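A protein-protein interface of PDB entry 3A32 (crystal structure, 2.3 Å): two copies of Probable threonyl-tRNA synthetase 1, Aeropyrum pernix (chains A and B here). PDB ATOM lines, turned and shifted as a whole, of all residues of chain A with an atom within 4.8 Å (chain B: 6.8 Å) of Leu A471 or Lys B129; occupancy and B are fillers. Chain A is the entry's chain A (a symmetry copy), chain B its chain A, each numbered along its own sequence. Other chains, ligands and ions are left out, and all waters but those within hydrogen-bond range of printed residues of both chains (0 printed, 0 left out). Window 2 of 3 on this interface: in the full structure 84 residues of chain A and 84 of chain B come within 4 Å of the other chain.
O of Phe A469 is in hydrogen-bond range of ND1 of His B126, at 3.5 Å.
NZ of Lys B129 lies close to O of Phe A469 (3.3 Å).
The side-chain amino group (NZ) of Lys B129 lies within hydrogen-bond range of the backbone carbonyl oxygen (O) of Leu A471 (2.8 Å).
Among the printed residues, pairs that only touch across the chains: Met A470 with His B126 (3.8 Å), Phe A469 with Leu B130 (3.9 Å) and Phe A469 with Pro B131 (3.98 Å).
Of the printed residues of chain B, Phe A469 touches His B126 (3.5 Å), Lys B129 (3.2 Å), Leu B130 (3.9 Å) and Pro B131 (3.98 Å).
Of the printed residues of chain B, Met A470 touches His B126 (3.8 Å).
Leu A471 touches just one residue of chain B: Lys B129 (2.8 Å).
Lys B125 touches none of the printed residues of chain A.
Lys B129 touches just these residues of chain A: Phe A469 (3.2 Å) and Leu A471 (2.8 Å).
Printed residues of chain A within 4 Å of Leu B130: Phe A469 (3.9 Å).
Of the printed residues of chain A, Pro B131 touches Phe A469 (3.98 Å).
The nearest residue of chain B that does not touch Leu A471 is His B126 (5.5 Å).
Of the 10 printed residues of chain B, 4 touch a printed residue of chain A.
Hydrophobic or aromatic side chains of chain B within 4 Å of the printed part of chain A: His B126, Leu B130 and Pro B131.
Along chain B the printed residues that touch a printed residue of chain A span positions 126 to 131.
Printed residues of chain A that touch a printed residue of chain B: Phe A469, Met A470 and Leu A471.
Among the printed residues, 6 pairs touch across the chains.
No position is printed for both chains.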
ATOM      1  N   ILE A 339      18.598  -6.580 -30.489  1.00  0.00           N
ATOM      2  CA  ILE A 339      18.288  -5.393 -29.672  1.00  0.00           C
ATOM      3  C   ILE A 339      17.391  -4.459 -30.485  1.00  0.00           C
ATOM      4  O   ILE A 339      17.806  -3.944 -31.539  1.00  0.00           O
ATOM      5  CB  ILE A 339      19.589  -4.652 -29.193  1.00  0.00           C
ATOM      6  CG1 ILE A 339      20.475  -5.603 -28.368  1.00  0.00           C
ATOM      7  CG2 ILE A 339      19.227  -3.367 -28.401  1.00  0.00           C
ATOM      8  CD1 ILE A 339      21.900  -5.034 -27.983  1.00  0.00           C
ATOM      9  N   ALA A 342      18.106   0.589 -28.325  1.00  0.00           N
ATOM     10  CA  ALA A 342      19.239   0.827 -27.433  1.00  0.00           C
ATOM     11  C   ALA A 342      19.006   2.212 -26.810  1.00  0.00           C
ATOM     12  O   ALA A 342      18.806   3.195 -27.552  1.00  0.00           O
ATOM     13  CB  ALA A 342      20.564   0.779 -28.170  1.00  0.00           C
ATOM     14  N   ALA A 375      18.315  -2.567 -24.630  1.00  0.00           N
ATOM     15  CA  ALA A 375      19.616  -2.519 -23.984  1.00  0.00           C
ATOM     16  C   ALA A 375      19.902  -1.065 -23.560  1.00  0.00           C
ATOM     17  O   ALA A 375      19.763  -0.144 -24.374  1.00  0.00           O
ATOM     18  CB  ALA A 375      20.691  -3.044 -24.935  1.00  0.00           C
ATOM     19  N   VAL A 376      20.248  -0.851 -22.289  1.00  0.00           N
ATOM     20  CA  VAL A 376      20.640   0.483 -21.793  1.00  0.00           C
ATOM     21  C   VAL A 376      22.143   0.541 -21.786  1.00  0.00           C
ATOM     22  O   VAL A 376      22.789  -0.420 -21.378  1.00  0.00           O
ATOM     23  CB  VAL A 376      20.160   0.723 -20.377  1.00  0.00           C
ATOM     24  CG1 VAL A 376      20.680   2.102 -19.850  1.00  0.00           C
ATOM     25  CG2 VAL A 376      18.670   0.691 -20.335  1.00  0.00           C
ATOM     26  N   LYS A 377      22.692   1.644 -22.281  1.00  0.00           N
ATOM     27  CA  LYS A 377      24.131   1.878 -22.220  1.00  0.00           C
ATOM     28  C   LYS A 377      24.389   3.190 -21.426  1.00  0.00           C
ATOM     29  O   LYS A 377      23.813   4.208 -21.722  1.00  0.00           O
ATOM     30  CB  LYS A 377      24.713   1.947 -23.644  1.00  0.00           C
ATOM     31  CG  LYS A 377      26.222   2.272 -23.772  1.00  0.00           C
ATOM     32  CD  LYS A 377      27.130   1.262 -23.011  1.00  0.00           C
ATOM     33  CE  LYS A 377      28.564   1.764 -23.051  1.00  0.00           C
ATOM     34  NZ  LYS A 377      29.556   0.725 -22.609  1.00  0.00           N
ATOM     35  N   ILE A 391      28.897   0.148 -30.436  1.00  0.00           N
ATOM     36  CA  ILE A 391      27.520  -0.272 -30.580  1.00  0.00           C
ATOM     37  C   ILE A 391      27.215  -0.548 -32.078  1.00  0.00           C
ATOM     38  O   ILE A 391      26.667  -1.583 -32.415  1.00  0.00           O
ATOM     39  CB  ILE A 391      26.578   0.777 -29.931  1.00  0.00           C
ATOM     40  CG1 ILE A 391      26.634   0.680 -28.413  1.00  0.00           C
ATOM     41  CG2 ILE A 391      25.153   0.640 -30.433  1.00  0.00           C
ATOM     42  CD1 ILE A 391      26.143   1.927 -27.697  1.00  0.00           C
ATOM     43  N   ALA A 395      26.654  -4.577 -31.943  1.00  0.00           N
ATOM     44  CA  ALA A 395      25.295  -4.888 -31.569  1.00  0.00           C
ATOM     45  C   ALA A 395      24.228  -4.428 -32.582  1.00  0.00           C
ATOM     46  O   ALA A 395      23.159  -5.078 -32.690  1.00  0.00           O
ATOM     47  CB  ALA A 395      25.001  -4.320 -30.220  1.00  0.00           C
ATOM     48  N   PHE A 467      18.885  -6.756 -22.831  1.00  0.00           N
ATOM     49  CA  PHE A 467      20.212  -7.112 -23.326  1.00  0.00           C
ATOM     50  C   PHE A 467      21.299  -6.065 -22.999  1.00  0.00           C
ATOM     51  O   PHE A 467      22.348  -6.004 -23.690  1.00  0.00           O
ATOM     52  CB  PHE A 467      20.143  -7.350 -24.834  1.00  0.00           C
ATOM     53  CG  PHE A 467      19.494  -8.653 -25.235  1.00  0.00           C
ATOM     54  CD1 PHE A 467      19.583  -9.795 -24.419  1.00  0.00           C
ATOM     55  CD2 PHE A 467      18.848  -8.755 -26.478  1.00  0.00           C
ATOM     56  CE1 PHE A 467      18.999 -11.035 -24.829  1.00  0.00           C
ATOM     57  CE2 PHE A 467      18.300  -9.980 -26.916  1.00  0.00           C
ATOM     58  CZ  PHE A 467      18.372 -11.124 -26.068  1.00  0.00           C
ATOM     59  N   SER A 468      21.073  -5.289 -21.930  1.00  0.00           N
ATOM     60  CA  SER A 468      22.014  -4.273 -21.498  1.00  0.00           C
ATOM     61  C   SER A 468      23.431  -4.818 -21.407  1.00  0.00           C
ATOM     62  O   SER A 468      24.343  -4.116 -21.795  1.00  0.00           O
ATOM     63  CB  SER A 468      21.635  -3.658 -20.151  1.00  0.00           C
ATOM     64  OG  SER A 468      20.329  -3.150 -20.190  1.00  0.00           O
ATOM     65  N   PHE A 469      23.603  -6.070 -20.958  1.00  0.00           N
ATOM     66  CA  PHE A 469      24.946  -6.652 -20.747  1.00  0.00           C
ATOM     67  C   PHE A 469      25.811  -6.684 -21.997  1.00  0.00           C
ATOM     68  O   PHE A 469      27.053  -6.762 -21.891  1.00  0.00           O
ATOM     69  CB  PHE A 469      24.855  -8.067 -20.129  1.00  0.00           C
ATOM     70  CG  PHE A 469      24.170  -9.081 -20.993  1.00  0.00           C
ATOM     71  CD1 PHE A 469      24.896  -9.833 -21.954  1.00  0.00           C
ATOM     72  CD2 PHE A 469      22.809  -9.342 -20.828  1.00  0.00           C
ATOM     73  CE1 PHE A 469      24.257 -10.817 -22.732  1.00  0.00           C
ATOM     74  CE2 PHE A 469      22.143 -10.331 -21.636  1.00  0.00           C
ATOM     75  CZ  PHE A 469      22.856 -11.051 -22.576  1.00  0.00           C
ATOM     76  N   MET A 470      25.142  -6.615 -23.170  1.00  0.00           N
ATOM     77  CA  MET A 470      25.778  -6.668 -24.485  1.00  0.00           C
ATOM     78  C   MET A 470      26.389  -5.338 -24.902  1.00  0.00           C
ATOM     79  O   MET A 470      27.176  -5.296 -25.848  1.00  0.00           O
ATOM     80  CB  MET A 470      24.758  -7.047 -25.566  1.00  0.00           C
ATOM     81  CG  MET A 470      24.152  -8.448 -25.437  1.00  0.00           C
ATOM     82  SD  MET A 470      23.135  -8.874 -26.903  1.00  0.00           S
ATOM     83  CE  MET A 470      22.645 -10.541 -26.407  1.00  0.00           C
ATOM     84  N   LEU A 471      26.023  -4.236 -24.244  1.00  0.00           N
ATOM     85  CA  LEU A 471      26.436  -2.933 -24.760  1.00  0.00           C
ATOM     86  C   LEU A 471      27.729  -2.360 -24.112  1.00  0.00           C
ATOM     87  O   LEU A 471      27.907  -2.572 -22.917  1.00  0.00           O
ATOM     88  CB  LEU A 471      25.259  -1.957 -24.713  1.00  0.00           C
ATOM     89  CG  LEU A 471      24.544  -1.716 -26.056  1.00  0.00           C
ATOM     90  CD1 LEU A 471      24.578  -2.857 -27.042  1.00  0.00           C
ATOM     91  CD2 LEU A 471      23.170  -1.134 -25.969  1.00  0.00           C
ATOM     92  N   LYS B 125      32.217 -13.624 -23.358  1.00  0.00           N
ATOM     93  CA  LYS B 125      32.015 -12.368 -24.066  1.00  0.00           C
ATOM     94  C   LYS B 125      31.853 -11.135 -23.148  1.00  0.00           C
ATOM     95  O   LYS B 125      32.467 -10.097 -23.415  1.00  0.00           O
ATOM     96  CB  LYS B 125      30.800 -12.545 -24.967  1.00  0.00           C
ATOM     97  CG  LYS B 125      31.078 -13.566 -26.110  1.00  0.00           C
ATOM     98  CD  LYS B 125      29.873 -13.777 -27.005  1.00  0.00           C
ATOM     99  CE  LYS B 125      29.569 -12.491 -27.761  1.00  0.00           C
ATOM    100  NZ  LYS B 125      28.429 -12.627 -28.698  1.00  0.00           N
ATOM    101  N   HIS B 126      31.045 -11.256 -22.068  1.00  0.00           N
ATOM    102  CA  HIS B 126      30.639 -10.111 -21.243  1.00  0.00           C
ATOM    103  C   HIS B 126      31.043 -10.179 -19.786  1.00  0.00           C
ATOM    104  O   HIS B 126      30.950  -9.185 -19.088  1.00  0.00           O
ATOM    105  CB  HIS B 126      29.128  -9.823 -21.413  1.00  0.00           C
ATOM    106  CG  HIS B 126      28.722  -9.743 -22.859  1.00  0.00           C
ATOM    107  ND1 HIS B 126      29.199  -8.768 -23.710  1.00  0.00           N
ATOM    108  CD2 HIS B 126      27.986 -10.583 -23.629  1.00  0.00           C
ATOM    109  CE1 HIS B 126      28.745  -8.985 -24.929  1.00  0.00           C
ATOM    110  NE2 HIS B 126      27.998 -10.072 -24.903  1.00  0.00           N
ATOM    111  N   ARG B 127      31.504 -11.342 -19.334  1.00  0.00           N
ATOM    112  CA  ARG B 127      32.014 -11.502 -17.961  1.00  0.00           C
ATOM    113  C   ARG B 127      30.908 -11.093 -17.002  1.00  0.00           C
ATOM    114  O   ARG B 127      29.731 -11.406 -17.260  1.00  0.00           O
ATOM    115  CB  ARG B 127      33.300 -10.688 -17.738  1.00  0.00           C
ATOM    116  CG  ARG B 127      34.325 -10.834 -18.877  1.00  0.00           C
ATOM    117  CD  ARG B 127      35.751 -11.015 -18.371  1.00  0.00           C
ATOM    118  NE  ARG B 127      36.619 -11.534 -19.444  1.00  0.00           N
ATOM    119  CZ  ARG B 127      36.579 -12.774 -19.961  1.00  0.00           C
ATOM    120  NH1 ARG B 127      35.702 -13.684 -19.526  1.00  0.00           N
ATOM    121  NH2 ARG B 127      37.428 -13.107 -20.930  1.00  0.00           N
ATOM    122  N   SER B 128      31.270 -10.360 -15.950  1.00  0.00           N
ATOM    123  CA  SER B 128      30.328  -9.986 -14.879  1.00  0.00           C
ATOM    124  C   SER B 128      29.272  -8.945 -15.247  1.00  0.00           C
ATOM    125  O   SER B 128      28.393  -8.657 -14.419  1.00  0.00           O
ATOM    126  CB  SER B 128      31.080  -9.516 -13.616  1.00  0.00           C
ATOM    127  OG  SER B 128      31.860  -8.381 -13.933  1.00  0.00           O
ATOM    128  N   LYS B 129      29.325  -8.364 -16.452  1.00  0.00           N
ATOM    129  CA  LYS B 129      28.154  -7.564 -16.923  1.00  0.00           C
ATOM    130  C   LYS B 129      26.885  -8.402 -17.062  1.00  0.00           C
ATOM    131  O   LYS B 129      25.764  -7.865 -16.984  1.00  0.00           O
ATOM    132  CB  LYS B 129      28.426  -6.884 -18.255  1.00  0.00           C
ATOM    133  CG  LYS B 129      29.481  -5.800 -18.228  1.00  0.00           C
ATOM    134  CD  LYS B 129      29.260  -4.911 -19.418  1.00  0.00           C
ATOM    135  CE  LYS B 129      29.767  -5.548 -20.678  1.00  0.00           C
ATOM    136  NZ  LYS B 129      29.519  -4.549 -21.772  1.00  0.00           N
ATOM    137  N   LEU B 130      27.063  -9.717 -17.269  1.00  0.00           N
ATOM    138  CA  LEU B 130      25.922 -10.653 -17.321  1.00  0.00           C
ATOM    139  C   LEU B 130      25.286 -10.659 -15.932  1.00  0.00           C
ATOM    140  O   LEU B 130      25.975 -10.962 -14.954  1.00  0.00           O
ATOM    141  CB  LEU B 130      26.356 -12.076 -17.676  1.00  0.00           C
ATOM    142  CG  LEU B 130      25.250 -13.094 -18.040  1.00  0.00           C
ATOM    143  CD1 LEU B 130      24.513 -12.745 -19.354  1.00  0.00           C
ATOM    144  CD2 LEU B 130      25.828 -14.480 -18.122  1.00  0.00           C
ATOM    145  N   PRO B 131      23.992 -10.300 -15.837  1.00  0.00           N
ATOM    146  CA  PRO B 131      23.365 -10.289 -14.522  1.00  0.00           C
ATOM    147  C   PRO B 131      23.051 -11.698 -13.960  1.00  0.00           C
ATOM    148  O   PRO B 131      22.825 -12.660 -14.709  1.00  0.00           O
ATOM    149  CB  PRO B 131      22.070  -9.487 -14.748  1.00  0.00           C
ATOM    150  CG  PRO B 131      22.057  -9.080 -16.179  1.00  0.00           C
ATOM    151  CD  PRO B 131      23.043  -9.920 -16.900  1.00  0.00           C
ATOM    152  N   LEU B 132      23.084 -11.807 -12.642  1.00  0.00           N
ATOM    153  CA  LEU B 132      22.593 -12.987 -11.956  1.00  0.00           C
ATOM    154  C   LEU B 132      21.423 -12.540 -11.076  1.00  0.00           C
ATOM    155  O   LEU B 132      21.447 -11.439 -10.534  1.00  0.00           O
ATOM    156  CB  LEU B 132      23.704 -13.605 -11.103  1.00  0.00           C
ATOM    157  CG  LEU B 132      24.973 -14.072 -11.806  1.00  0.00           C
ATOM    158  CD1 LEU B 132      26.007 -14.636 -10.818  1.00  0.00           C
ATOM    159  CD2 LEU B 132      24.669 -15.110 -12.978  1.00  0.00           C
ATOM    160  N   GLU B 300      34.753 -14.836 -11.940  1.00  0.00           N
ATOM    161  CA  GLU B 300      34.148 -13.717 -12.675  1.00  0.00           C
ATOM    162  C   GLU B 300      33.185 -12.867 -11.860  1.00  0.00           C
ATOM    163  O   GLU B 300      33.102 -11.662 -12.073  1.00  0.00           O
ATOM    164  CB  GLU B 300      33.423 -14.214 -13.926  1.00  0.00           C
ATOM    165  CG  GLU B 300      34.279 -14.998 -14.926  1.00  0.00           C
ATOM    166  CD  GLU B 300      35.435 -14.180 -15.513  1.00  0.00           C
ATOM    167  OE1 GLU B 300      35.358 -12.931 -15.565  1.00  0.00           O
ATOM    168  OE2 GLU B 300      36.441 -14.793 -15.923  1.00  0.00           O
ATOM    169  N   PHE B 301      32.433 -13.469 -10.940  1.00  0.00           N
ATOM    170  CA  PHE B 301      31.450 -12.686 -10.185  1.00  0.00           C
ATOM    171  C   PHE B 301      31.812 -12.480  -8.715  1.00  0.00           C
ATOM    172  O   PHE B 301      31.155 -11.697  -8.020  1.00  0.00           O
ATOM    173  CB  PHE B 301      30.030 -13.273 -10.305  1.00  0.00           C
ATOM    174  CG  PHE B 301      29.550 -13.430 -11.705  1.00  0.00           C
ATOM    175  CD1 PHE B 301      28.650 -12.531 -12.235  1.00  0.00           C
ATOM    176  CD2 PHE B 301      29.967 -14.505 -12.487  1.00  0.00           C
ATOM    177  CE1 PHE B 301      28.190 -12.670 -13.566  1.00  0.00           C
ATOM    178  CE2 PHE B 301      29.502 -14.670 -13.811  1.00  0.00           C
ATOM    179  CZ  PHE B 301      28.625 -13.753 -14.346  1.00  0.00           C
